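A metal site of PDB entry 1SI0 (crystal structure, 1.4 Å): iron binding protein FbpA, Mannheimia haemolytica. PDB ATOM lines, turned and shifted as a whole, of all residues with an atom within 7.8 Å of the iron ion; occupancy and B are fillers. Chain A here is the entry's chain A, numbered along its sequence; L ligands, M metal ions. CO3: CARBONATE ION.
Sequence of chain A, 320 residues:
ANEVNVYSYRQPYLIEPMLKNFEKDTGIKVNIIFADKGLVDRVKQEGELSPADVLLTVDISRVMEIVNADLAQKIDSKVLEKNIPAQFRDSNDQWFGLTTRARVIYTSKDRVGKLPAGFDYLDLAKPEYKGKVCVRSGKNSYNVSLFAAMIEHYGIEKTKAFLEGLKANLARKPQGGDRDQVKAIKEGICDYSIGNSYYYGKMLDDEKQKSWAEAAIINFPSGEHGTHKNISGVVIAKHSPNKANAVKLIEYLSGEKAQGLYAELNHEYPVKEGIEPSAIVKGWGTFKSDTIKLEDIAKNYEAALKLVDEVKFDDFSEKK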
ATOM      1  N   TYR A   9      12.005 -14.539  -5.361  1.00  0.00           N
ATOM      2  CA  TYR A   9      10.973 -14.619  -6.391  1.00  0.00           C
ATOM      3  C   TYR A   9       9.759 -13.779  -6.030  1.00  0.00           C
ATOM      4  O   TYR A   9       8.898 -13.546  -6.878  1.00  0.00           O
ATOM      5  CB  TYR A   9      10.520 -16.066  -6.585  1.00  0.00           C
ATOM      6  CG  TYR A   9      11.463 -16.905  -7.422  1.00  0.00           C
ATOM      7  CD1 TYR A   9      11.442 -16.804  -8.798  1.00  0.00           C
ATOM      8  CD2 TYR A   9      12.335 -17.801  -6.828  1.00  0.00           C
ATOM      9  CE1 TYR A   9      12.295 -17.574  -9.591  1.00  0.00           C
ATOM     10  CE2 TYR A   9      13.187 -18.584  -7.616  1.00  0.00           C
ATOM     11  CZ  TYR A   9      13.157 -18.451  -8.991  1.00  0.00           C
ATOM     12  OH  TYR A   9      13.990 -19.210  -9.782  1.00  0.00           O
ATOM     13  N   ARG A  10       9.645 -13.380  -4.766  1.00  0.00           N
ATOM     14  CA  ARG A  10       8.571 -12.490  -4.373  1.00  0.00           C
ATOM     15  C   ARG A  10       8.798 -11.128  -4.954  1.00  0.00           C
ATOM     16  O   ARG A  10       9.947 -10.676  -5.094  1.00  0.00           O
ATOM     17  CB  ARG A  10       8.481 -12.383  -2.868  1.00  0.00           C
ATOM     18  CG  ARG A  10       8.179 -13.713  -2.204  1.00  0.00           C
ATOM     19  CD  ARG A  10       7.056 -13.694  -1.225  1.00  0.00           C
ATOM     20  NE  ARG A  10       5.818 -13.119  -1.759  1.00  0.00           N
ATOM     21  CZ  ARG A  10       4.734 -12.982  -1.021  1.00  0.00           C
ATOM     22  NH1 ARG A  10       3.643 -12.457  -1.543  1.00  0.00           N
ATOM     23  NH2 ARG A  10       4.740 -13.401   0.237  1.00  0.00           N
ATOM     24  N   GLN A  11       7.711 -10.447  -5.273  1.00  0.00           N
ATOM     25  CA  GLN A  11       7.792  -9.079  -5.755  1.00  0.00           C
ATOM     26  C   GLN A  11       8.166  -8.163  -4.613  1.00  0.00           C
ATOM     27  O   GLN A  11       7.746  -8.368  -3.475  1.00  0.00           O
ATOM     28  CB  GLN A  11       6.460  -8.657  -6.336  1.00  0.00           C
ATOM     29  CG  GLN A  11       6.081  -9.504  -7.516  1.00  0.00           C
ATOM     30  CD  GLN A  11       4.791  -9.071  -8.122  1.00  0.00           C
ATOM     31  OE1 GLN A  11       4.742  -8.070  -8.816  1.00  0.00           O
ATOM     32  NE2 GLN A  11       3.734  -9.822  -7.857  1.00  0.00           N
ATOM     33  N   TYR A  13       7.135  -5.281  -3.548  1.00  0.00           N
ATOM     34  CA  TYR A  13       6.054  -4.694  -2.748  1.00  0.00           C
ATOM     35  C   TYR A  13       5.377  -5.671  -1.799  1.00  0.00           C
ATOM     36  O   TYR A  13       4.711  -5.260  -0.843  1.00  0.00           O
ATOM     37  CB  TYR A  13       5.034  -3.968  -3.637  1.00  0.00           C
ATOM     38  CG  TYR A  13       4.013  -4.832  -4.354  1.00  0.00           C
ATOM     39  CD1 TYR A  13       4.365  -5.596  -5.466  1.00  0.00           C
ATOM     40  CD2 TYR A  13       2.695  -4.824  -3.956  1.00  0.00           C
ATOM     41  CE1 TYR A  13       3.415  -6.360  -6.137  1.00  0.00           C
ATOM     42  CE2 TYR A  13       1.746  -5.579  -4.624  1.00  0.00           C
ATOM     43  CZ  TYR A  13       2.106  -6.333  -5.709  1.00  0.00           C
ATOM     44  OH  TYR A  13       1.147  -7.072  -6.360  1.00  0.00           O
ATOM     45  N   LEU A  14       5.564  -6.965  -2.044  1.00  0.00           N
ATOM     46  CA  LEU A  14       4.992  -8.033  -1.220  1.00  0.00           C
ATOM     47  C   LEU A  14       5.970  -8.693  -0.253  1.00  0.00           C
ATOM     48  O   LEU A  14       5.611  -9.642   0.429  1.00  0.00           O
ATOM     49  CB  LEU A  14       4.387  -9.092  -2.134  1.00  0.00           C
ATOM     50  CG  LEU A  14       3.182  -8.588  -2.922  1.00  0.00           C
ATOM     51  CD1 LEU A  14       2.857  -9.524  -4.068  1.00  0.00           C
ATOM     52  CD2 LEU A  14       1.969  -8.400  -2.011  1.00  0.00           C
ATOM     53  N   VAL A  58       7.446 -18.131  -4.357  1.00  0.00           N
ATOM     54  CA  VAL A  58       6.004 -17.926  -4.419  1.00  0.00           C
ATOM     55  C   VAL A  58       5.261 -19.182  -4.839  1.00  0.00           C
ATOM     56  O   VAL A  58       4.091 -19.122  -5.165  1.00  0.00           O
ATOM     57  CB  VAL A  58       5.636 -16.777  -5.390  1.00  0.00           C
ATOM     58  CG1 VAL A  58       6.166 -15.452  -4.894  1.00  0.00           C
ATOM     59  CG2 VAL A  58       6.106 -17.042  -6.810  1.00  0.00           C
ATOM     60  N   ARG A 101      -1.915 -19.131  -0.188  1.00  0.00           N
ATOM     61  CA  ARG A 101      -2.700 -18.289  -1.078  1.00  0.00           C
ATOM     62  C   ARG A 101      -3.577 -19.215  -1.884  1.00  0.00           C
ATOM     63  O   ARG A 101      -3.268 -20.384  -2.070  1.00  0.00           O
ATOM     64  CB  ARG A 101      -1.810 -17.457  -1.994  1.00  0.00           C
ATOM     65  CG  ARG A 101      -0.719 -18.219  -2.733  1.00  0.00           C
ATOM     66  CD  ARG A 101       0.608 -18.263  -2.022  1.00  0.00           C
ATOM     67  NE  ARG A 101       1.240 -16.949  -1.878  1.00  0.00           N
ATOM     68  CZ  ARG A 101       1.876 -16.281  -2.835  1.00  0.00           C
ATOM     69  NH1 ARG A 101       2.404 -15.104  -2.560  1.00  0.00           N
ATOM     70  NH2 ARG A 101       1.985 -16.757  -4.066  1.00  0.00           N
ATOM     71  N   ARG A 103      -5.544 -19.794  -5.585  1.00  0.00           N
ATOM     72  CA  ARG A 103      -5.662 -19.338  -6.956  1.00  0.00           C
ATOM     73  C   ARG A 103      -7.127 -19.426  -7.310  1.00  0.00           C
ATOM     74  O   ARG A 103      -7.690 -20.505  -7.451  1.00  0.00           O
ATOM     75  CB  ARG A 103      -4.791 -20.156  -7.897  1.00  0.00           C
ATOM     76  CG  ARG A 103      -4.613 -19.524  -9.261  1.00  0.00           C
ATOM     77  CD  ARG A 103      -3.241 -19.789  -9.877  1.00  0.00           C
ATOM     78  NE  ARG A 103      -3.025 -19.003 -11.090  1.00  0.00           N
ATOM     79  CZ  ARG A 103      -2.735 -17.705 -11.108  1.00  0.00           C
ATOM     80  NH1 ARG A 103      -2.581 -17.095 -12.256  1.00  0.00           N
ATOM     81  NH2 ARG A 103      -2.589 -17.028  -9.983  1.00  0.00           N
ATOM     82  N   ARG A 136      -3.107 -14.821 -17.412  1.00  0.00           N
ATOM     83  CA  ARG A 136      -1.724 -14.502 -17.685  1.00  0.00           C
ATOM     84  C   ARG A 136      -1.038 -15.710 -18.322  1.00  0.00           C
ATOM     85  O   ARG A 136      -1.622 -16.777 -18.438  1.00  0.00           O
ATOM     86  CB  ARG A 136      -0.996 -14.103 -16.421  1.00  0.00           C
ATOM     87  CG  ARG A 136      -0.634 -15.267 -15.521  1.00  0.00           C
ATOM     88  CD  ARG A 136      -0.132 -14.866 -14.176  1.00  0.00           C
ATOM     89  NE  ARG A 136       1.114 -14.102 -14.237  1.00  0.00           N
ATOM     90  CZ  ARG A 136       1.644 -13.479 -13.201  1.00  0.00           C
ATOM     91  NH1 ARG A 136       1.038 -13.506 -12.017  1.00  0.00           N
ATOM     92  NH2 ARG A 136       2.771 -12.811 -13.343  1.00  0.00           N
ATOM     93  N   ASN A 140       3.490 -19.118 -16.444  1.00  0.00           N
ATOM     94  CA  ASN A 140       3.692 -18.533 -15.146  1.00  0.00           C
ATOM     95  C   ASN A 140       3.506 -19.621 -14.095  1.00  0.00           C
ATOM     96  O   ASN A 140       2.580 -20.421 -14.196  1.00  0.00           O
ATOM     97  CB  ASN A 140       2.716 -17.393 -14.894  1.00  0.00           C
ATOM     98  CG  ASN A 140       2.715 -16.941 -13.470  1.00  0.00           C
ATOM     99  OD1 ASN A 140       1.896 -17.400 -12.680  1.00  0.00           O
ATOM    100  ND2 ASN A 140       3.658 -16.069 -13.123  1.00  0.00           N
ATOM    101  N   TYR A 142       2.361 -19.827 -11.134  1.00  0.00           N
ATOM    102  CA  TYR A 142       1.080 -19.956 -10.452  1.00  0.00           C
ATOM    103  C   TYR A 142       0.119 -20.792 -11.294  1.00  0.00           C
ATOM    104  O   TYR A 142      -0.596 -21.636 -10.780  1.00  0.00           O
ATOM    105  CB  TYR A 142       0.425 -18.598 -10.218  1.00  0.00           C
ATOM    106  CG  TYR A 142       1.165 -17.658  -9.308  1.00  0.00           C
ATOM    107  CD1 TYR A 142       1.945 -18.113  -8.253  1.00  0.00           C
ATOM    108  CD2 TYR A 142       1.036 -16.278  -9.467  1.00  0.00           C
ATOM    109  CE1 TYR A 142       2.567 -17.241  -7.412  1.00  0.00           C
ATOM    110  CE2 TYR A 142       1.668 -15.396  -8.621  1.00  0.00           C
ATOM    111  CZ  TYR A 142       2.428 -15.884  -7.592  1.00  0.00           C
ATOM    112  OH  TYR A 142       3.049 -15.006  -6.738  1.00  0.00           O
ATOM    113  N   ASP A 178      -1.570 -11.126 -12.657  1.00  0.00           N
ATOM    114  CA  ASP A 178      -2.897 -11.451 -12.156  1.00  0.00           C
ATOM    115  C   ASP A 178      -3.782 -10.212 -12.019  1.00  0.00           C
ATOM    116  O   ASP A 178      -4.945 -10.254 -12.363  1.00  0.00           O
ATOM    117  CB  ASP A 178      -2.797 -12.149 -10.797  1.00  0.00           C
ATOM    118  CG  ASP A 178      -2.434 -13.610 -10.901  1.00  0.00           C
ATOM    119  OD1 ASP A 178      -2.345 -14.172 -12.027  1.00  0.00           O
ATOM    120  OD2 ASP A 178      -2.263 -14.266  -9.865  1.00  0.00           O
ATOM    121  N   ASN A 196      -4.336 -15.005  -8.097  1.00  0.00           N
ATOM    122  CA  ASN A 196      -4.205 -15.324  -6.691  1.00  0.00           C
ATOM    123  C   ASN A 196      -5.064 -14.398  -5.857  1.00  0.00           C
ATOM    124  O   ASN A 196      -5.270 -13.241  -6.209  1.00  0.00           O
ATOM    125  CB  ASN A 196      -2.756 -15.245  -6.235  1.00  0.00           C
ATOM    126  CG  ASN A 196      -1.930 -16.430  -6.689  1.00  0.00           C
ATOM    127  OD1 ASN A 196      -2.459 -17.435  -7.177  1.00  0.00           O
ATOM    128  ND2 ASN A 196      -0.624 -16.336  -6.508  1.00  0.00           N
ATOM    129  N   TYR A 198      -4.719 -12.967  -2.805  1.00  0.00           N
ATOM    130  CA  TYR A 198      -4.189 -11.805  -2.092  1.00  0.00           C
ATOM    131  C   TYR A 198      -4.137 -10.563  -2.984  1.00  0.00           C
ATOM    132  O   TYR A 198      -4.257  -9.449  -2.481  1.00  0.00           O
ATOM    133  CB  TYR A 198      -2.806 -12.090  -1.452  1.00  0.00           C
ATOM    134  CG  TYR A 198      -1.821 -12.621  -2.442  1.00  0.00           C
ATOM    135  CD1 TYR A 198      -1.745 -13.979  -2.711  1.00  0.00           C
ATOM    136  CD2 TYR A 198      -0.965 -11.765  -3.123  1.00  0.00           C
ATOM    137  CE1 TYR A 198      -0.854 -14.464  -3.625  1.00  0.00           C
ATOM    138  CE2 TYR A 198      -0.083 -12.245  -4.047  1.00  0.00           C
ATOM    139  CZ  TYR A 198      -0.038 -13.606  -4.309  1.00  0.00           C
ATOM    140  OH  TYR A 198       0.803 -14.135  -5.244  1.00  0.00           O
ATOM    141  N   TYR A 199      -4.003 -10.751  -4.291  1.00  0.00           N
ATOM    142  CA  TYR A 199      -4.003  -9.598  -5.201  1.00  0.00           C
ATOM    143  C   TYR A 199      -5.302  -8.814  -5.127  1.00  0.00           C
ATOM    144  O   TYR A 199      -5.293  -7.603  -5.353  1.00  0.00           O
ATOM    145  CB  TYR A 199      -3.738 -10.004  -6.639  1.00  0.00           C
ATOM    146  CG  TYR A 199      -2.342 -10.533  -6.841  1.00  0.00           C
ATOM    147  CD1 TYR A 199      -2.129 -11.811  -7.315  1.00  0.00           C
ATOM    148  CD2 TYR A 199      -1.228  -9.752  -6.539  1.00  0.00           C
ATOM    149  CE1 TYR A 199      -0.844 -12.306  -7.490  1.00  0.00           C
ATOM    150  CE2 TYR A 199       0.048 -10.238  -6.710  1.00  0.00           C
ATOM    151  CZ  TYR A 199       0.240 -11.515  -7.186  1.00  0.00           C
ATOM    152  OH  TYR A 199       1.515 -11.999  -7.335  1.00  0.00           O
ATOM    153  N   SER A 232       3.761 -19.277  -0.294  1.00  0.00           N
ATOM    154  CA  SER A 232       5.054 -18.618  -0.362  1.00  0.00           C
ATOM    155  C   SER A 232       5.938 -19.397   0.582  1.00  0.00           C
ATOM    156  O   SER A 232       5.495 -19.883   1.617  1.00  0.00           O
ATOM    157  CB  SER A 232       4.986 -17.139   0.010  1.00  0.00           C
ATOM    158  OG  SER A 232       4.887 -16.914   1.410  1.00  0.00           O
ATOM    159  N   GLU A 268      -2.520 -12.174   2.447  1.00  0.00           N
ATOM    160  CA  GLU A 268      -2.295 -13.604   2.323  1.00  0.00           C
ATOM    161  C   GLU A 268      -2.811 -14.288   3.586  1.00  0.00           C
ATOM    162  O   GLU A 268      -3.120 -13.651   4.584  1.00  0.00           O
ATOM    163  CB  GLU A 268      -0.811 -13.874   2.146  1.00  0.00           C
ATOM    164  CG  GLU A 268      -0.309 -13.453   0.787  1.00  0.00           C
ATOM    165  CD  GLU A 268       1.145 -13.753   0.606  1.00  0.00           C
ATOM    166  OE1 GLU A 268       1.451 -14.875   0.169  1.00  0.00           O
ATOM    167  OE2 GLU A 268       1.981 -12.871   0.906  1.00  0.00           O
HETATM  168  C   CO3 L   1       4.401 -12.389  -4.979  1.00  0.00           C
HETATM  169  O1  CO3 L   1       3.428 -12.938  -4.334  1.00  0.00           O
HETATM  170  O2  CO3 L   1       4.315 -12.282  -6.261  1.00  0.00           O
HETATM  171  O3  CO3 L   1       5.440 -11.978  -4.345  1.00  0.00           O
HETATM  172 FE    FE M   1       2.362 -13.301  -6.107  1.00  0.00          FE
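NH2 of Arg 101 lies close to OH of Tyr 142. N of Tyr 142 lies within hydrogen-bond range of OD1 of Asn 140, at 2.9 Å. OH of Tyr 198 lies close to NH2 of Arg 101 (3.1 Å). The side-chain hydroxyl (OH) of Tyr 198 sits close to the side-chain amide nitrogen (ND2) of Asn 196, at 2.9 Å. The side-chain hydroxyl (OH) of Tyr 199 sits close to the side-chain amide nitrogen (NE2) of Gln 11 (3.2 Å). The guanidinium group (NH2) of Arg 101 lies within hydrogen-bond range of the backbone carbonyl oxygen (O) of Val 58. The guanidinium group of Arg 101 is in salt-bridge range of the side-chain carboxylate of Glu 268 (2.9 Å).
Arg 101 touches the iron ion (NH1 to FE, 3.98 Å). Four residues have an atom within 4 Å of the iron ion: Arg 101, Tyr 142, Tyr 198 and Tyr 199. Along chain A the residues within 4 Å of the iron ion span positions 101 to 199. The nearest printed residue that does not touch the iron ion is Gln 11 (4.1 Å).
The iron ion is bound by the side-chain hydroxyl (OH) of Tyr 142 (1.9 Å), the side-chain hydroxyl (OH) of Tyr 198 (2.0 Å), the side-chain hydroxyl (OH) of Tyr 199 (2.0 Å), an oxygen (O1) of the ligand (2.1 Å) and an oxygen (O2) of the ligand (2.2 Å).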
